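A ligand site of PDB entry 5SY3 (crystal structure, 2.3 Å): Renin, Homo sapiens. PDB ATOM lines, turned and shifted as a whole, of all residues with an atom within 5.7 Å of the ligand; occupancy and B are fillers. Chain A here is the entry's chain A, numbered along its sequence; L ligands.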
ATOM      1  N   THR A  17      29.802   7.153  16.978  1.00  0.00           N
ATOM      2  CA  THR A  17      30.271   7.535  18.312  1.00  0.00           C
ATOM      3  C   THR A  17      29.298   8.404  19.104  1.00  0.00           C
ATOM      4  O   THR A  17      29.452   8.512  20.308  1.00  0.00           O
ATOM      5  CB  THR A  17      31.586   8.300  18.236  1.00  0.00           C
ATOM      6  OG1 THR A  17      31.401   9.487  17.461  1.00  0.00           O
ATOM      7  CG2 THR A  17      32.680   7.421  17.608  1.00  0.00           C
ATOM      8  N   GLN A  18      28.318   9.032  18.442  1.00  0.00           N
ATOM      9  CA  GLN A  18      27.299   9.797  19.145  1.00  0.00           C
ATOM     10  C   GLN A  18      25.959   9.468  18.537  1.00  0.00           C
ATOM     11  O   GLN A  18      25.797   9.496  17.311  1.00  0.00           O
ATOM     12  CB  GLN A  18      27.551  11.301  19.037  1.00  0.00           C
ATOM     13  CG  GLN A  18      28.889  11.720  19.616  1.00  0.00           C
ATOM     14  CD  GLN A  18      29.185  13.194  19.407  1.00  0.00           C
ATOM     15  OE1 GLN A  18      28.285  14.037  19.404  1.00  0.00           O
ATOM     16  NE2 GLN A  18      30.463  13.514  19.253  1.00  0.00           N
ATOM     17  N   TYR A  19      25.006   9.163  19.418  1.00  0.00           N
ATOM     18  CA  TYR A  19      23.643   8.868  19.060  1.00  0.00           C
ATOM     19  C   TYR A  19      22.774   9.776  19.883  1.00  0.00           C
ATOM     20  O   TYR A  19      22.913   9.837  21.100  1.00  0.00           O
ATOM     21  CB  TYR A  19      23.297   7.416  19.352  1.00  0.00           C
ATOM     22  CG  TYR A  19      24.039   6.421  18.479  1.00  0.00           C
ATOM     23  CD1 TYR A  19      25.337   6.028  18.799  1.00  0.00           C
ATOM     24  CD2 TYR A  19      23.458   5.885  17.337  1.00  0.00           C
ATOM     25  CE1 TYR A  19      26.025   5.121  18.008  1.00  0.00           C
ATOM     26  CE2 TYR A  19      24.134   4.980  16.534  1.00  0.00           C
ATOM     27  CZ  TYR A  19      25.426   4.604  16.879  1.00  0.00           C
ATOM     28  OH  TYR A  19      26.121   3.706  16.107  1.00  0.00           O
ATOM     29  N   TYR A  20      21.869  10.486  19.216  1.00  0.00           N
ATOM     30  CA  TYR A  20      21.028  11.462  19.884  1.00  0.00           C
ATOM     31  C   TYR A  20      19.752  11.677  19.095  1.00  0.00           C
ATOM     32  O   TYR A  20      19.715  11.485  17.877  1.00  0.00           O
ATOM     33  CB  TYR A  20      21.795  12.788  20.067  1.00  0.00           C
ATOM     34  CG  TYR A  20      22.555  13.235  18.837  1.00  0.00           C
ATOM     35  CD1 TYR A  20      21.963  14.050  17.878  1.00  0.00           C
ATOM     36  CD2 TYR A  20      23.871  12.821  18.628  1.00  0.00           C
ATOM     37  CE1 TYR A  20      22.655  14.452  16.749  1.00  0.00           C
ATOM     38  CE2 TYR A  20      24.576  13.217  17.502  1.00  0.00           C
ATOM     39  CZ  TYR A  20      23.963  14.031  16.562  1.00  0.00           C
ATOM     40  OH  TYR A  20      24.656  14.429  15.455  1.00  0.00           O
ATOM     41  N   VAL A  35      21.445  13.199  23.995  1.00  0.00           N
ATOM     42  CA  VAL A  35      21.852  11.817  24.202  1.00  0.00           C
ATOM     43  C   VAL A  35      20.956  11.246  25.287  1.00  0.00           C
ATOM     44  O   VAL A  35      20.767  11.875  26.325  1.00  0.00           O
ATOM     45  CB  VAL A  35      23.325  11.701  24.646  1.00  0.00           C
ATOM     46  CG1 VAL A  35      23.696  10.274  25.021  1.00  0.00           C
ATOM     47  CG2 VAL A  35      24.244  12.210  23.551  1.00  0.00           C
ATOM     48  N   ASP A  37      21.027   8.740  27.938  1.00  0.00           N
ATOM     49  CA  ASP A  37      22.231   8.199  28.577  1.00  0.00           C
ATOM     50  C   ASP A  37      21.885   7.355  29.808  1.00  0.00           C
ATOM     51  O   ASP A  37      21.546   7.898  30.855  1.00  0.00           O
ATOM     52  CB  ASP A  37      23.154   9.363  28.965  1.00  0.00           C
ATOM     53  CG  ASP A  37      24.398   8.919  29.747  1.00  0.00           C
ATOM     54  OD1 ASP A  37      24.890   7.794  29.569  1.00  0.00           O
ATOM     55  OD2 ASP A  37      24.887   9.730  30.552  1.00  0.00           O
ATOM     56  N   SER A  40      23.871   7.995  33.286  1.00  0.00           N
ATOM     57  CA  SER A  40      23.576   9.111  34.193  1.00  0.00           C
ATOM     58  C   SER A  40      22.064   9.275  34.341  1.00  0.00           C
ATOM     59  O   SER A  40      21.300   8.573  33.692  1.00  0.00           O
ATOM     60  CB  SER A  40      24.198  10.391  33.660  1.00  0.00           C
ATOM     61  OG  SER A  40      23.610  10.763  32.427  1.00  0.00           O
ATOM     62  N   TRP A  44      19.539  17.729  31.216  1.00  0.00           N
ATOM     63  CA  TRP A  44      19.932  19.114  31.002  1.00  0.00           C
ATOM     64  C   TRP A  44      20.060  19.453  29.524  1.00  0.00           C
ATOM     65  O   TRP A  44      20.245  18.576  28.678  1.00  0.00           O
ATOM     66  CB  TRP A  44      21.238  19.450  31.730  1.00  0.00           C
ATOM     67  CG  TRP A  44      22.442  18.702  31.233  1.00  0.00           C
ATOM     68  CD1 TRP A  44      22.932  17.529  31.723  1.00  0.00           C
ATOM     69  CD2 TRP A  44      23.307  19.070  30.144  1.00  0.00           C
ATOM     70  NE1 TRP A  44      24.045  17.143  31.009  1.00  0.00           N
ATOM     71  CE2 TRP A  44      24.298  18.066  30.038  1.00  0.00           C
ATOM     72  CE3 TRP A  44      23.324  20.141  29.238  1.00  0.00           C
ATOM     73  CZ2 TRP A  44      25.314  18.114  29.065  1.00  0.00           C
ATOM     74  CZ3 TRP A  44      24.343  20.180  28.267  1.00  0.00           C
ATOM     75  CH2 TRP A  44      25.315  19.169  28.193  1.00  0.00           C
ATOM     76  N   TYR A  82      30.996  14.234  34.212  1.00  0.00           N
ATOM     77  CA  TYR A  82      31.019  13.020  33.378  1.00  0.00           C
ATOM     78  C   TYR A  82      32.450  12.557  33.166  1.00  0.00           C
ATOM     79  O   TYR A  82      33.401  13.242  33.567  1.00  0.00           O
ATOM     80  CB  TYR A  82      30.353  13.286  32.021  1.00  0.00           C
ATOM     81  CG  TYR A  82      28.897  13.676  32.148  1.00  0.00           C
ATOM     82  CD1 TYR A  82      27.922  12.712  32.419  1.00  0.00           C
ATOM     83  CD2 TYR A  82      28.480  14.999  31.978  1.00  0.00           C
ATOM     84  CE1 TYR A  82      26.590  13.053  32.532  1.00  0.00           C
ATOM     85  CE2 TYR A  82      27.144  15.350  32.088  1.00  0.00           C
ATOM     86  CZ  TYR A  82      26.198  14.366  32.368  1.00  0.00           C
ATOM     87  OH  TYR A  82      24.869  14.698  32.485  1.00  0.00           O
ATOM     88  N   THR A  84      34.006  12.261  30.275  1.00  0.00           N
ATOM     89  CA  THR A  84      34.632  13.099  29.246  1.00  0.00           C
ATOM     90  C   THR A  84      34.651  14.602  29.576  1.00  0.00           C
ATOM     91  O   THR A  84      35.452  15.341  29.007  1.00  0.00           O
ATOM     92  CB  THR A  84      33.975  12.880  27.840  1.00  0.00           C
ATOM     93  OG1 THR A  84      32.580  12.557  27.982  1.00  0.00           O
ATOM     94  CG2 THR A  84      34.695  11.742  27.093  1.00  0.00           C
ATOM     95  N   GLY A  85      33.789  15.059  30.485  1.00  0.00           N
ATOM     96  CA  GLY A  85      33.718  16.485  30.817  1.00  0.00           C
ATOM     97  C   GLY A  85      32.735  16.897  31.885  1.00  0.00           C
ATOM     98  O   GLY A  85      31.937  16.088  32.349  1.00  0.00           O
ATOM     99  N   PRO A 117      34.502  18.667  26.426  1.00  0.00           N
ATOM    100  CA  PRO A 117      34.285  18.010  25.130  1.00  0.00           C
ATOM    101  C   PRO A 117      33.147  18.601  24.273  1.00  0.00           C
ATOM    102  O   PRO A 117      32.845  18.060  23.206  1.00  0.00           O
ATOM    103  CB  PRO A 117      33.861  16.598  25.558  1.00  0.00           C
ATOM    104  CG  PRO A 117      33.037  16.869  26.792  1.00  0.00           C
ATOM    105  CD  PRO A 117      33.724  18.008  27.488  1.00  0.00           C
ATOM    106  N   PHE A 118      32.506  19.669  24.735  1.00  0.00           N
ATOM    107  CA  PHE A 118      31.230  20.059  24.125  1.00  0.00           C
ATOM    108  C   PHE A 118      31.321  20.728  22.761  1.00  0.00           C
ATOM    109  O   PHE A 118      30.325  20.764  22.059  1.00  0.00           O
ATOM    110  CB  PHE A 118      30.363  20.817  25.130  1.00  0.00           C
ATOM    111  CG  PHE A 118      29.994  19.976  26.294  1.00  0.00           C
ATOM    112  CD1 PHE A 118      29.035  18.969  26.169  1.00  0.00           C
ATOM    113  CD2 PHE A 118      30.679  20.091  27.504  1.00  0.00           C
ATOM    114  CE1 PHE A 118      28.723  18.146  27.229  1.00  0.00           C
ATOM    115  CE2 PHE A 118      30.382  19.257  28.579  1.00  0.00           C
ATOM    116  CZ  PHE A 118      29.401  18.279  28.433  1.00  0.00           C
ATOM    117  N   LEU A 120      32.987  19.190  20.475  1.00  0.00           N
ATOM    118  CA  LEU A 120      32.879  17.984  19.645  1.00  0.00           C
ATOM    119  C   LEU A 120      31.567  17.209  19.851  1.00  0.00           C
ATOM    120  O   LEU A 120      31.373  16.176  19.221  1.00  0.00           O
ATOM    121  CB  LEU A 120      34.123  17.076  19.769  1.00  0.00           C
ATOM    122  CG  LEU A 120      34.595  16.471  21.103  1.00  0.00           C
ATOM    123  CD1 LEU A 120      33.694  15.335  21.572  1.00  0.00           C
ATOM    124  CD2 LEU A 120      36.021  15.990  20.938  1.00  0.00           C
ATOM    125  N   ALA A 121      30.667  17.711  20.700  1.00  0.00           N
ATOM    126  CA  ALA A 121      29.339  17.122  20.879  1.00  0.00           C
ATOM    127  C   ALA A 121      28.409  17.697  19.819  1.00  0.00           C
ATOM    128  O   ALA A 121      28.191  18.918  19.756  1.00  0.00           O
ATOM    129  CB  ALA A 121      28.792  17.424  22.261  1.00  0.00           C
ATOM    130  N   PHE A 123      25.305  16.923  19.749  1.00  0.00           N
ATOM    131  CA  PHE A 123      24.067  17.070  20.491  1.00  0.00           C
ATOM    132  C   PHE A 123      24.177  18.299  21.388  1.00  0.00           C
ATOM    133  O   PHE A 123      25.277  18.814  21.627  1.00  0.00           O
ATOM    134  CB  PHE A 123      23.792  15.802  21.302  1.00  0.00           C
ATOM    135  CG  PHE A 123      24.891  15.433  22.255  1.00  0.00           C
ATOM    136  CD1 PHE A 123      25.939  14.589  21.843  1.00  0.00           C
ATOM    137  CD2 PHE A 123      24.905  15.946  23.550  1.00  0.00           C
ATOM    138  CE1 PHE A 123      26.957  14.264  22.720  1.00  0.00           C
ATOM    139  CE2 PHE A 123      25.924  15.618  24.419  1.00  0.00           C
ATOM    140  CZ  PHE A 123      26.949  14.780  24.013  1.00  0.00           C
ATOM    141  N   VAL A 126      21.556  16.246  27.427  1.00  0.00           N
ATOM    142  CA  VAL A 126      21.543  14.876  27.920  1.00  0.00           C
ATOM    143  C   VAL A 126      20.255  14.613  28.666  1.00  0.00           C
ATOM    144  O   VAL A 126      19.815  15.457  29.462  1.00  0.00           O
ATOM    145  CB  VAL A 126      22.727  14.595  28.877  1.00  0.00           C
ATOM    146  CG1 VAL A 126      22.707  13.154  29.370  1.00  0.00           C
ATOM    147  CG2 VAL A 126      24.057  14.917  28.191  1.00  0.00           C
ATOM    148  N   TYR A 161      20.796   1.162  18.089  1.00  0.00           N
ATOM    149  CA  TYR A 161      21.814   1.981  17.457  1.00  0.00           C
ATOM    150  C   TYR A 161      22.215   1.325  16.147  1.00  0.00           C
ATOM    151  O   TYR A 161      22.714   0.212  16.156  1.00  0.00           O
ATOM    152  CB  TYR A 161      23.053   2.096  18.361  1.00  0.00           C
ATOM    153  CG  TYR A 161      22.951   3.036  19.555  1.00  0.00           C
ATOM    154  CD1 TYR A 161      21.876   3.921  19.730  1.00  0.00           C
ATOM    155  CD2 TYR A 161      23.956   3.060  20.513  1.00  0.00           C
ATOM    156  CE1 TYR A 161      21.823   4.786  20.815  1.00  0.00           C
ATOM    157  CE2 TYR A 161      23.904   3.925  21.599  1.00  0.00           C
ATOM    158  CZ  TYR A 161      22.840   4.780  21.742  1.00  0.00           C
ATOM    159  OH  TYR A 161      22.778   5.639  22.818  1.00  0.00           O
ATOM    160  N   THR A 226      24.421   3.675  27.437  1.00  0.00           N
ATOM    161  CA  THR A 226      23.964   4.124  26.122  1.00  0.00           C
ATOM    162  C   THR A 226      24.584   5.470  25.683  1.00  0.00           C
ATOM    163  O   THR A 226      24.513   5.828  24.502  1.00  0.00           O
ATOM    164  CB  THR A 226      22.437   4.245  26.070  1.00  0.00           C
ATOM    165  OG1 THR A 226      22.015   5.213  27.040  1.00  0.00           O
ATOM    166  CG2 THR A 226      21.763   2.900  26.344  1.00  0.00           C
ATOM    167  N   GLY A 227      25.159   6.194  26.630  1.00  0.00           N
ATOM    168  CA  GLY A 227      25.872   7.435  26.339  1.00  0.00           C
ATOM    169  C   GLY A 227      27.380   7.308  26.169  1.00  0.00           C
ATOM    170  O   GLY A 227      28.060   8.319  26.093  1.00  0.00           O
ATOM    171  N   ALA A 228      27.883   6.067  26.165  1.00  0.00           N
ATOM    172  CA  ALA A 228      29.297   5.764  25.913  1.00  0.00           C
ATOM    173  C   ALA A 228      29.429   5.258  24.484  1.00  0.00           C
ATOM    174  O   ALA A 228      28.606   4.456  24.027  1.00  0.00           O
ATOM    175  CB  ALA A 228      29.799   4.703  26.874  1.00  0.00           C
ATOM    176  N   SER A 229      30.479   5.702  23.803  1.00  0.00           N
ATOM    177  CA  SER A 229      30.704   5.379  22.412  1.00  0.00           C
ATOM    178  C   SER A 229      31.180   3.951  22.252  1.00  0.00           C
ATOM    179  O   SER A 229      30.826   3.292  21.289  1.00  0.00           O
ATOM    180  CB  SER A 229      31.753   6.315  21.790  1.00  0.00           C
ATOM    181  OG  SER A 229      31.310   7.651  21.813  1.00  0.00           O
ATOM    182  N   ALA A 316      28.085   2.033  22.788  1.00  0.00           N
ATOM    183  CA  ALA A 316      27.442   1.950  21.468  1.00  0.00           C
ATOM    184  C   ALA A 316      27.957   0.790  20.620  1.00  0.00           C
ATOM    185  O   ALA A 316      27.198   0.189  19.867  1.00  0.00           O
ATOM    186  CB  ALA A 316      27.581   3.268  20.721  1.00  0.00           C
HETATM  187  C1  LIG L   1      31.140  13.287  23.313  1.00  0.00           C
HETATM  188  C2  LIG L   1      30.168  13.873  25.349  1.00  0.00           C
HETATM  189  C3  LIG L   1      27.877  13.793  28.683  1.00  0.00           C
HETATM  190  C4  LIG L   1      27.576  11.438  26.826  1.00  0.00           C
HETATM  191  C5  LIG L   1      29.402  12.691  25.352  1.00  0.00           C
HETATM  192  C6  LIG L   1      26.558   9.365  22.940  1.00  0.00           C
HETATM  193  C7  LIG L   1      29.084   9.573  23.224  1.00  0.00           C
HETATM  194  N1  LIG L   1      28.849  10.640  24.184  1.00  0.00           N
HETATM  195  C8  LIG L   1      29.573  11.823  24.229  1.00  0.00           C
HETATM  196  N2  LIG L   1      30.436  12.166  23.263  1.00  0.00           N
HETATM  197  N3  LIG L   1      31.010  14.130  24.323  1.00  0.00           N
HETATM  198  S1  LIG L   1      29.813  14.805  26.790  1.00  0.00           S
HETATM  199  C9  LIG L   1      28.662  13.629  27.380  1.00  0.00           C
HETATM  200  C10 LIG L   1      27.029  12.545  29.002  1.00  0.00           C
HETATM  201  C11 LIG L   1      26.440  11.915  27.730  1.00  0.00           C
HETATM  202  C12 LIG L   1      28.543  12.595  26.537  1.00  0.00           C
HETATM  203  C13 LIG L   1      27.800   8.835  22.959  1.00  0.00           C
HETATM  204  C14 LIG L   1      25.680   8.309  22.650  1.00  0.00           C
HETATM  205  C15 LIG L   1      26.414   7.193  22.497  1.00  0.00           C
HETATM  206  O1  LIG L   1      27.703   7.515  22.691  1.00  0.00           O
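A nitrogen (N1) of the ligand sits at hydrogen-bond distance from the backbone carbonyl oxygen of Gly 227 (3.1 Å).
The backbone NH (N) of Ser 229 sits at hydrogen-bond distance from an oxygen (O1) of the ligand, at 3.5 Å.
A sulfur (S1) of the ligand lies close to the side-chain hydroxyl of Thr 84, at 3.8 Å.
O of Thr 226 is in hydrogen-bond range of OH of Tyr 161 (2.4 Å).
The backbone NH of Gly 227 sits at hydrogen-bond distance from the side-chain carboxylate of Asp 37 (3.4 Å).
O of Thr 17 lies within hydrogen-bond range of OG of Ser 229 (2.5 Å).
O of Ser 229 sits close to N of Ala 316, 3.4 Å away.
The backbone NH (N) of Ala 316 is in hydrogen-bond range of the backbone carbonyl oxygen (O) of Ala 228, at 2.8 Å.
The indole nitrogen (NE1) of Trp 44 lies within hydrogen-bond range of the side-chain hydroxyl (OH) of Tyr 82.
The side-chain amide nitrogen (NE2) of Gln 18 is in hydrogen-bond range of the backbone carbonyl oxygen (O) of Leu 120, at 2.8 Å.
The side-chain carboxylate of Asp 37 lies within hydrogen-bond range of the side-chain hydroxyl of Ser 40 (2.5 Å).
O of Thr 17 sits close to O1 of the ligand (3.1 Å).
The backbone carbonyl oxygen of Ala 228 lies close to an oxygen (O1) of the ligand (3.5 Å).
CA of Gln 18 touches C6 of the ligand (3.9 Å).
Tyr 19 touches the ligand (N to C14, 3.4 Å).
CG1 of Val 35 touches C6 of the ligand (3.7 Å).
OD2 of Asp 37 touches C10 of the ligand (3.9 Å).
Tyr 82 touches the ligand.
CG of Pro 117 touches S1 of the ligand, 3.8 Å away.
Phe 118 touches the ligand (CE1 to S1, 3.5 Å).
Leu 120 touches the ligand.
Phe 123 touches the ligand.
Val 126 touches the ligand (CG2 to C11, 3.9 Å).
Tyr 161 touches the ligand.
Thr 226 touches the ligand (O to C15, 3.1 Å).
Hydrophobic or aromatic side chains that line the ligand: Val 35, Tyr 82, Pro 117, Phe 118, Leu 120, Phe 123 and Val 126.
Within 4 Å of the ligand: Thr 17, Gln 18, Tyr 19, Val 35, Asp 37, Tyr 82, Thr 84, Pro 117, Phe 118, Leu 120, Phe 123, Val 126, Tyr 161, Thr 226, Gly 227, Ala 228 and Ser 229.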
